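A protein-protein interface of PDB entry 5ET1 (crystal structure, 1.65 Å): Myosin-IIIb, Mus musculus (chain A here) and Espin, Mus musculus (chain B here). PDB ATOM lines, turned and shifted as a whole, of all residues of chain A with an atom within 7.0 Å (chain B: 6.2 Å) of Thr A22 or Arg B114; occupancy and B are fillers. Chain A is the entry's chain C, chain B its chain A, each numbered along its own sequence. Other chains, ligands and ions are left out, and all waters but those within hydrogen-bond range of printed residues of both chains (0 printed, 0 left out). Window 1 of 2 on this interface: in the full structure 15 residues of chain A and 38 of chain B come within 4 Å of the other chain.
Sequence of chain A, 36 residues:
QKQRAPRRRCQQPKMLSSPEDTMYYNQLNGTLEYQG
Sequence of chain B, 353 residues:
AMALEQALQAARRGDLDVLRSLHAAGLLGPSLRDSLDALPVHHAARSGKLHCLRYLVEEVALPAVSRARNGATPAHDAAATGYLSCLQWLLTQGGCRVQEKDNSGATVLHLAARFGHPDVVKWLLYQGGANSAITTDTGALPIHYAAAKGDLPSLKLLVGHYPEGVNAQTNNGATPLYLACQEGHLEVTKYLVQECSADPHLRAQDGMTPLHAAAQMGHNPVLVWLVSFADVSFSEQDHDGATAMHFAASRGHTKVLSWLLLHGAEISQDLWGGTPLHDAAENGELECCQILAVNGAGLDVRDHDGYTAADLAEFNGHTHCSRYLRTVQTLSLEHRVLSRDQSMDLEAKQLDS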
ATOM      1  N   MET A  15      11.974  19.286  15.500  1.00  0.00           N
ATOM      2  CA  MET A  15      11.578  20.678  15.565  1.00  0.00           C
ATOM      3  C   MET A  15      11.050  21.123  14.207  1.00  0.00           C
ATOM      4  O   MET A  15      11.470  20.622  13.162  1.00  0.00           O
ATOM      5  CB  MET A  15      12.757  21.546  16.013  1.00  0.00           C
ATOM      6  CG  MET A  15      13.006  21.427  17.519  1.00  0.00           C
ATOM      7  SD  MET A  15      14.593  22.075  18.077  1.00  0.00           S
ATOM      8  CE  MET A  15      14.911  23.365  16.867  1.00  0.00           C
ATOM      9  N   LEU A  16      10.093  22.038  14.242  1.00  0.00           N
ATOM     10  CA  LEU A  16       9.477  22.562  13.027  1.00  0.00           C
ATOM     11  C   LEU A  16      10.141  23.837  12.526  1.00  0.00           C
ATOM     12  O   LEU A  16       9.962  24.190  11.356  1.00  0.00           O
ATOM     13  CB  LEU A  16       7.991  22.833  13.275  1.00  0.00           C
ATOM     14  CG  LEU A  16       7.139  21.629  13.695  1.00  0.00           C
ATOM     15  CD1 LEU A  16       5.744  22.081  14.133  1.00  0.00           C
ATOM     16  CD2 LEU A  16       7.057  20.607  12.559  1.00  0.00           C
ATOM     17  N   SER A  17      10.889  24.540  13.380  1.00  0.00           N
ATOM     18  CA  SER A  17      11.590  25.753  12.980  1.00  0.00           C
ATOM     19  C   SER A  17      13.042  25.677  13.428  1.00  0.00           C
ATOM     20  O   SER A  17      13.438  24.805  14.205  1.00  0.00           O
ATOM     21  CB  SER A  17      10.938  27.011  13.566  1.00  0.00           C
ATOM     22  OG  SER A  17      11.190  27.124  14.951  1.00  0.00           O
ATOM     23  N   SER A  18      13.833  26.627  12.946  1.00  0.00           N
ATOM     24  CA  SER A  18      15.211  26.743  13.369  1.00  0.00           C
ATOM     25  C   SER A  18      15.291  27.245  14.809  1.00  0.00           C
ATOM     26  O   SER A  18      14.360  27.882  15.307  1.00  0.00           O
ATOM     27  CB  SER A  18      15.957  27.718  12.465  1.00  0.00           C
ATOM     28  OG  SER A  18      15.429  29.020  12.635  1.00  0.00           O
ATOM     29  N   PRO A  19      16.411  26.979  15.491  1.00  0.00           N
ATOM     30  CA  PRO A  19      16.585  27.533  16.846  1.00  0.00           C
ATOM     31  C   PRO A  19      16.562  29.053  16.872  1.00  0.00           C
ATOM     32  O   PRO A  19      16.032  29.657  17.815  1.00  0.00           O
ATOM     33  CB  PRO A  19      17.956  26.984  17.277  1.00  0.00           C
ATOM     34  CG  PRO A  19      18.228  25.835  16.376  1.00  0.00           C
ATOM     35  CD  PRO A  19      17.539  26.121  15.085  1.00  0.00           C
ATOM     36  N   GLU A  20      17.133  29.692  15.849  1.00  0.00           N
ATOM     37  CA  GLU A  20      17.125  31.149  15.791  1.00  0.00           C
ATOM     38  C   GLU A  20      15.697  31.677  15.701  1.00  0.00           C
ATOM     39  O   GLU A  20      15.345  32.682  16.334  1.00  0.00           O
ATOM     40  CB  GLU A  20      17.989  31.608  14.605  1.00  0.00           C
ATOM     41  CG  GLU A  20      19.473  31.216  14.733  1.00  0.00           C
ATOM     42  CD  GLU A  20      19.804  29.800  14.237  1.00  0.00           C
ATOM     43  OE1 GLU A  20      18.877  29.025  13.908  1.00  0.00           O
ATOM     44  OE2 GLU A  20      21.010  29.461  14.177  1.00  0.00           O
ATOM     45  N   ASP A  21      14.852  30.966  14.953  1.00  0.00           N
ATOM     46  CA  ASP A  21      13.431  31.297  14.843  1.00  0.00           C
ATOM     47  C   ASP A  21      12.727  31.150  16.182  1.00  0.00           C
ATOM     48  O   ASP A  21      11.942  32.010  16.598  1.00  0.00           O
ATOM     49  CB  ASP A  21      12.757  30.360  13.836  1.00  0.00           C
ATOM     50  CG  ASP A  21      12.448  31.015  12.520  1.00  0.00           C
ATOM     51  OD1 ASP A  21      12.549  32.253  12.411  1.00  0.00           O
ATOM     52  OD2 ASP A  21      12.080  30.270  11.590  1.00  0.00           O
ATOM     53  N   THR A  22      12.963  30.026  16.854  1.00  0.00           N
ATOM     54  CA  THR A  22      12.331  29.784  18.143  1.00  0.00           C
ATOM     55  C   THR A  22      12.759  30.824  19.167  1.00  0.00           C
ATOM     56  O   THR A  22      11.941  31.317  19.953  1.00  0.00           O
ATOM     57  CB  THR A  22      12.687  28.375  18.609  1.00  0.00           C
ATOM     58  OG1 THR A  22      12.168  27.434  17.657  1.00  0.00           O
ATOM     59  CG2 THR A  22      12.115  28.099  19.991  1.00  0.00           C
ATOM     60  N   MET A  23      14.046  31.178  19.166  1.00  0.00           N
ATOM     61  CA  MET A  23      14.521  32.227  20.056  1.00  0.00           C
ATOM     62  C   MET A  23      13.749  33.522  19.826  1.00  0.00           C
ATOM     63  O   MET A  23      13.272  34.150  20.776  1.00  0.00           O
ATOM     64  CB  MET A  23      16.027  32.424  19.851  1.00  0.00           C
ATOM     65  CG  MET A  23      16.666  33.490  20.750  1.00  0.00           C
ATOM     66  SD  MET A  23      16.486  35.154  20.072  1.00  0.00           S
ATOM     67  CE  MET A  23      17.584  35.032  18.641  1.00  0.00           C
ATOM     68  N   TYR A  24      13.591  33.925  18.563  1.00  0.00           N
ATOM     69  CA  TYR A  24      12.907  35.187  18.283  1.00  0.00           C
ATOM     70  C   TYR A  24      11.457  35.152  18.767  1.00  0.00           C
ATOM     71  O   TYR A  24      10.994  36.070  19.459  1.00  0.00           O
ATOM     72  CB  TYR A  24      12.931  35.497  16.782  1.00  0.00           C
ATOM     73  CG  TYR A  24      12.135  36.748  16.480  1.00  0.00           C
ATOM     74  CD1 TYR A  24      10.796  36.674  16.095  1.00  0.00           C
ATOM     75  CD2 TYR A  24      12.708  38.009  16.627  1.00  0.00           C
ATOM     76  CE1 TYR A  24      10.061  37.825  15.848  1.00  0.00           C
ATOM     77  CE2 TYR A  24      11.981  39.165  16.389  1.00  0.00           C
ATOM     78  CZ  TYR A  24      10.652  39.061  16.002  1.00  0.00           C
ATOM     79  OH  TYR A  24       9.938  40.211  15.745  1.00  0.00           O
ATOM     80  N   TYR A  25      10.708  34.121  18.375  1.00  0.00           N
ATOM     81  CA  TYR A  25       9.294  34.125  18.746  1.00  0.00           C
ATOM     82  C   TYR A  25       9.112  33.921  20.241  1.00  0.00           C
ATOM     83  O   TYR A  25       8.150  34.440  20.826  1.00  0.00           O
ATOM     84  CB  TYR A  25       8.529  33.090  17.909  1.00  0.00           C
ATOM     85  CG  TYR A  25       8.396  33.519  16.462  1.00  0.00           C
ATOM     86  CD1 TYR A  25       7.668  34.663  16.123  1.00  0.00           C
ATOM     87  CD2 TYR A  25       9.000  32.798  15.436  1.00  0.00           C
ATOM     88  CE1 TYR A  25       7.536  35.074  14.821  1.00  0.00           C
ATOM     89  CE2 TYR A  25       8.872  33.207  14.100  1.00  0.00           C
ATOM     90  CZ  TYR A  25       8.152  34.351  13.809  1.00  0.00           C
ATOM     91  OH  TYR A  25       8.005  34.766  12.515  1.00  0.00           O
ATOM     92  N   ASN A  26      10.050  33.224  20.896  1.00  0.00           N
ATOM     93  CA  ASN A  26       9.959  33.094  22.345  1.00  0.00           C
ATOM     94  C   ASN A  26      10.232  34.407  23.073  1.00  0.00           C
ATOM     95  O   ASN A  26       9.777  34.567  24.208  1.00  0.00           O
ATOM     96  CB  ASN A  26      10.927  32.028  22.861  1.00  0.00           C
ATOM     97  CG  ASN A  26      10.430  30.607  22.620  1.00  0.00           C
ATOM     98  OD1 ASN A  26       9.301  30.393  22.194  1.00  0.00           O
ATOM     99  ND2 ASN A  26      11.280  29.622  22.928  1.00  0.00           N
ATOM    100  N   GLN A  27      10.998  35.339  22.484  1.00  0.00           N
ATOM    101  CA  GLN A  27      11.290  36.571  23.209  1.00  0.00           C
ATOM    102  C   GLN A  27      10.275  37.672  22.934  1.00  0.00           C
ATOM    103  O   GLN A  27      10.518  38.823  23.302  1.00  0.00           O
ATOM    104  CB  GLN A  27      12.719  37.070  22.929  1.00  0.00           C
ATOM    105  CG  GLN A  27      13.096  37.345  21.491  1.00  0.00           C
ATOM    106  CD  GLN A  27      12.684  38.743  20.996  1.00  0.00           C
ATOM    107  OE1 GLN A  27      13.068  39.772  21.563  1.00  0.00           O
ATOM    108  NE2 GLN A  27      11.919  38.774  19.913  1.00  0.00           N
ATOM    109  N   LEU B 109      -0.727  32.367   9.740  1.00  0.00           N
ATOM    110  CA  LEU B 109      -1.501  31.187  10.126  1.00  0.00           C
ATOM    111  C   LEU B 109      -0.631  30.143  10.823  1.00  0.00           C
ATOM    112  O   LEU B 109      -1.067  29.526  11.802  1.00  0.00           O
ATOM    113  CB  LEU B 109      -2.188  30.576   8.901  1.00  0.00           C
ATOM    114  CG  LEU B 109      -3.074  29.353   9.159  1.00  0.00           C
ATOM    115  CD1 LEU B 109      -4.250  29.671  10.101  1.00  0.00           C
ATOM    116  CD2 LEU B 109      -3.605  28.806   7.849  1.00  0.00           C
ATOM    117  N   HIS B 110       0.589  29.905  10.320  1.00  0.00           N
ATOM    118  CA  HIS B 110       1.497  28.998  11.031  1.00  0.00           C
ATOM    119  C   HIS B 110       1.742  29.465  12.455  1.00  0.00           C
ATOM    120  O   HIS B 110       1.756  28.654  13.387  1.00  0.00           O
ATOM    121  CB  HIS B 110       2.855  28.890  10.330  1.00  0.00           C
ATOM    122  CG  HIS B 110       2.828  28.158   9.028  1.00  0.00           C
ATOM    123  ND1 HIS B 110       2.654  28.799   7.822  1.00  0.00           N
ATOM    124  CD2 HIS B 110       3.042  26.851   8.735  1.00  0.00           C
ATOM    125  CE1 HIS B 110       2.721  27.914   6.842  1.00  0.00           C
ATOM    126  NE2 HIS B 110       2.949  26.721   7.369  1.00  0.00           N
ATOM    127  N   LEU B 111       1.979  30.765  12.633  1.00  0.00           N
ATOM    128  CA  LEU B 111       2.387  31.252  13.945  1.00  0.00           C
ATOM    129  C   LEU B 111       1.218  31.266  14.921  1.00  0.00           C
ATOM    130  O   LEU B 111       1.404  30.992  16.122  1.00  0.00           O
ATOM    131  CB  LEU B 111       2.997  32.642  13.815  1.00  0.00           C
ATOM    132  CG  LEU B 111       4.262  32.695  12.965  1.00  0.00           C
ATOM    133  CD1 LEU B 111       4.685  34.122  12.833  1.00  0.00           C
ATOM    134  CD2 LEU B 111       5.380  31.854  13.572  1.00  0.00           C
ATOM    135  N   ALA B 112       0.013  31.591  14.434  1.00  0.00           N
ATOM    136  CA  ALA B 112      -1.172  31.516  15.291  1.00  0.00           C
ATOM    137  C   ALA B 112      -1.389  30.096  15.793  1.00  0.00           C
ATOM    138  O   ALA B 112      -1.764  29.889  16.952  1.00  0.00           O
ATOM    139  CB  ALA B 112      -2.405  32.006  14.525  1.00  0.00           C
ATOM    140  N   ALA B 113      -1.160  29.108  14.929  1.00  0.00           N
ATOM    141  CA  ALA B 113      -1.272  27.713  15.336  1.00  0.00           C
ATOM    142  C   ALA B 113      -0.149  27.333  16.286  1.00  0.00           C
ATOM    143  O   ALA B 113      -0.383  26.665  17.299  1.00  0.00           O
ATOM    144  CB  ALA B 113      -1.252  26.817  14.098  1.00  0.00           C
ATOM    145  N   ARG B 114       1.076  27.783  15.981  1.00  0.00           N
ATOM    146  CA  ARG B 114       2.243  27.418  16.785  1.00  0.00           C
ATOM    147  C   ARG B 114       2.067  27.802  18.242  1.00  0.00           C
ATOM    148  O   ARG B 114       2.511  27.078  19.146  1.00  0.00           O
ATOM    149  CB  ARG B 114       3.491  28.097  16.214  1.00  0.00           C
ATOM    150  CG  ARG B 114       4.716  27.921  17.070  1.00  0.00           C
ATOM    151  CD  ARG B 114       6.019  28.518  16.462  1.00  0.00           C
ATOM    152  NE  ARG B 114       7.082  28.203  17.412  1.00  0.00           N
ATOM    153  CZ  ARG B 114       8.387  28.251  17.161  1.00  0.00           C
ATOM    154  NH1 ARG B 114       8.836  28.633  15.971  1.00  0.00           N
ATOM    155  NH2 ARG B 114       9.242  27.906  18.119  1.00  0.00           N
ATOM    156  N   PHE B 115       1.453  28.952  18.493  1.00  0.00           N
ATOM    157  CA  PHE B 115       1.357  29.476  19.844  1.00  0.00           C
ATOM    158  C   PHE B 115      -0.042  29.355  20.409  1.00  0.00           C
ATOM    159  O   PHE B 115      -0.326  29.914  21.480  1.00  0.00           O
ATOM    160  CB  PHE B 115       1.872  30.919  19.885  1.00  0.00           C
ATOM    161  CG  PHE B 115       3.367  30.988  19.749  1.00  0.00           C
ATOM    162  CD1 PHE B 115       4.176  30.631  20.812  1.00  0.00           C
ATOM    163  CD2 PHE B 115       3.959  31.322  18.544  1.00  0.00           C
ATOM    164  CE1 PHE B 115       5.560  30.651  20.687  1.00  0.00           C
ATOM    165  CE2 PHE B 115       5.334  31.334  18.410  1.00  0.00           C
ATOM    166  CZ  PHE B 115       6.132  31.001  19.485  1.00  0.00           C
ATOM    167  N   GLY B 116      -0.911  28.605  19.738  1.00  0.00           N
ATOM    168  CA  GLY B 116      -2.182  28.214  20.330  1.00  0.00           C
ATOM    169  C   GLY B 116      -3.197  29.327  20.487  1.00  0.00           C
ATOM    170  O   GLY B 116      -3.763  29.525  21.576  1.00  0.00           O
ATOM    171  N   HIS B 117      -3.458  30.056  19.399  1.00  0.00           N
ATOM    172  CA  HIS B 117      -4.395  31.180  19.415  1.00  0.00           C
ATOM    173  C   HIS B 117      -5.546  30.886  18.469  1.00  0.00           C
ATOM    174  O   HIS B 117      -5.551  31.350  17.321  1.00  0.00           O
ATOM    175  CB  HIS B 117      -3.678  32.470  19.038  1.00  0.00           C
ATOM    176  CG  HIS B 117      -2.570  32.810  19.977  1.00  0.00           C
ATOM    177  ND1 HIS B 117      -2.764  32.923  21.335  1.00  0.00           N
ATOM    178  CD2 HIS B 117      -1.259  33.073  19.753  1.00  0.00           C
ATOM    179  CE1 HIS B 117      -1.614  33.236  21.911  1.00  0.00           C
ATOM    180  NE2 HIS B 117      -0.689  33.336  20.972  1.00  0.00           N
ATOM    181  N   PRO B 142       0.414  24.472   8.893  1.00  0.00           N
ATOM    182  CA  PRO B 142      -0.181  24.961  10.147  1.00  0.00           C
ATOM    183  C   PRO B 142      -0.668  23.816  11.031  1.00  0.00           C
ATOM    184  O   PRO B 142      -0.521  23.888  12.255  1.00  0.00           O
ATOM    185  CB  PRO B 142      -1.321  25.866   9.647  1.00  0.00           C
ATOM    186  CG  PRO B 142      -0.758  26.410   8.311  1.00  0.00           C
ATOM    187  CD  PRO B 142      -0.118  25.171   7.706  1.00  0.00           C
ATOM    188  N   TYR B 145       1.904  22.583  13.419  1.00  0.00           N
ATOM    189  CA  TYR B 145       2.124  23.478  14.554  1.00  0.00           C
ATOM    190  C   TYR B 145       1.007  23.361  15.582  1.00  0.00           C
ATOM    191  O   TYR B 145       1.267  23.381  16.793  1.00  0.00           O
ATOM    192  CB  TYR B 145       2.239  24.916  14.060  1.00  0.00           C
ATOM    193  CG  TYR B 145       3.640  25.296  13.630  1.00  0.00           C
ATOM    194  CD1 TYR B 145       4.667  25.400  14.568  1.00  0.00           C
ATOM    195  CD2 TYR B 145       3.939  25.546  12.296  1.00  0.00           C
ATOM    196  CE1 TYR B 145       5.962  25.756  14.195  1.00  0.00           C
ATOM    197  CE2 TYR B 145       5.232  25.901  11.909  1.00  0.00           C
ATOM    198  CZ  TYR B 145       6.228  26.014  12.866  1.00  0.00           C
ATOM    199  OH  TYR B 145       7.493  26.372  12.499  1.00  0.00           O
ATOM    200  N   ALA B 146      -0.242  23.277  15.122  1.00  0.00           N
ATOM    201  CA  ALA B 146      -1.352  23.155  16.061  1.00  0.00           C
ATOM    202  C   ALA B 146      -1.256  21.859  16.859  1.00  0.00           C
ATOM    203  O   ALA B 146      -1.532  21.840  18.067  1.00  0.00           O
ATOM    204  CB  ALA B 146      -2.678  23.225  15.310  1.00  0.00           C
ATOM    205  N   ALA B 148       1.557  20.132  17.536  1.00  0.00           N
ATOM    206  CA  ALA B 148       2.675  20.214  18.462  1.00  0.00           C
ATOM    207  C   ALA B 148       2.339  21.079  19.666  1.00  0.00           C
ATOM    208  O   ALA B 148       2.832  20.822  20.764  1.00  0.00           O
ATOM    209  CB  ALA B 148       3.919  20.761  17.747  1.00  0.00           C
ATOM    210  N   LYS B 149       1.523  22.118  19.476  1.00  0.00           N
ATOM    211  CA  LYS B 149       1.104  22.973  20.580  1.00  0.00           C
ATOM    212  C   LYS B 149       0.053  22.302  21.465  1.00  0.00           C
ATOM    213  O   LYS B 149      -0.080  22.664  22.637  1.00  0.00           O
ATOM    214  CB  LYS B 149       0.566  24.304  20.017  1.00  0.00           C
ATOM    215  CG  LYS B 149       0.019  25.294  21.044  1.00  0.00           C
ATOM    216  CD  LYS B 149       1.067  25.737  22.054  1.00  0.00           C
ATOM    217  CE  LYS B 149       0.431  26.620  23.125  1.00  0.00           C
ATOM    218  NZ  LYS B 149       1.345  26.806  24.288  1.00  0.00           N
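The backbone carbonyl oxygen of Phe B115 is in hydrogen-bond range of a ring nitrogen (NE2) of His B117, 3.5 Å away.
The side-chain hydroxyl (OG) of Ser A17 lies within hydrogen-bond range of the side-chain hydroxyl (OG1) of Thr A22, at 2.9 Å.
The backbone carbonyl oxygen (O) of Ser A18 lies within hydrogen-bond range of the side-chain hydroxyl (OG1) of Thr A22 (3.2 Å).
The side-chain amide nitrogen (ND2) of Asn A26 sits close to the backbone carbonyl oxygen (O) of Thr A22.
Printed residues of chain B within 4 Å of Leu A16: Tyr B145 (3.5 Å).
Of chain B, only Arg B114 (3.0 Å) comes within 4 Å of Thr A22.
Of the printed residues of chain B, Tyr A25 touches Leu B111 (3.4 Å) and Phe B115 (3.5 Å).
Of the printed residues of chain A, Leu B111 touches Tyr A25 (3.4 Å).
Printed residues of chain A within 4 Å of Arg B114: Ser A17 (3.0 Å) and Thr A22 (3.0 Å).
The nearest residue of chain B that does not touch Thr A22 is Phe B115 (5.8 Å).
Of the 13 printed residues of chain A, 4 touch a printed residue of chain B.
Hydrophobic or aromatic side chains of chain A within 4 Å of the printed part of chain B: Leu A16 and Tyr A25.
Of the 14 printed residues of chain B, 4 touch a printed residue of chain A.
Printed residues of chain B that touch a printed residue of chain A: Leu B111, Arg B114, Phe B115 and Tyr B145.
Hydrophobic or aromatic side chains of chain B within 4 Å of the printed part of chain A: Leu B111, Phe B115 and Tyr B145.
Among the printed residues, no Asp or Glu carboxylate lies within 4 Å of a Lys or Arg side-chain nitrogen of the other chain.
Tyr B145 touches Ser A17.
Tyr A25 touches Leu B111 (OH to CD1, 3.4 Å).
Tyr A25 touches Phe B115 (CB to CZ, 3.5 Å).
The guanidinium group of Arg B114 is in hydrogen-bond range of the side-chain hydroxyl of Ser A17, 3.0 Å away.
The guanidinium group (NH2) of Arg B114 sits at hydrogen-bond distance from the side-chain hydroxyl (OG1) of Thr A22 (3.0 Å).
OH of Tyr B145 is in hydrogen-bond range of O of Leu A16, at 3.5 Å.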
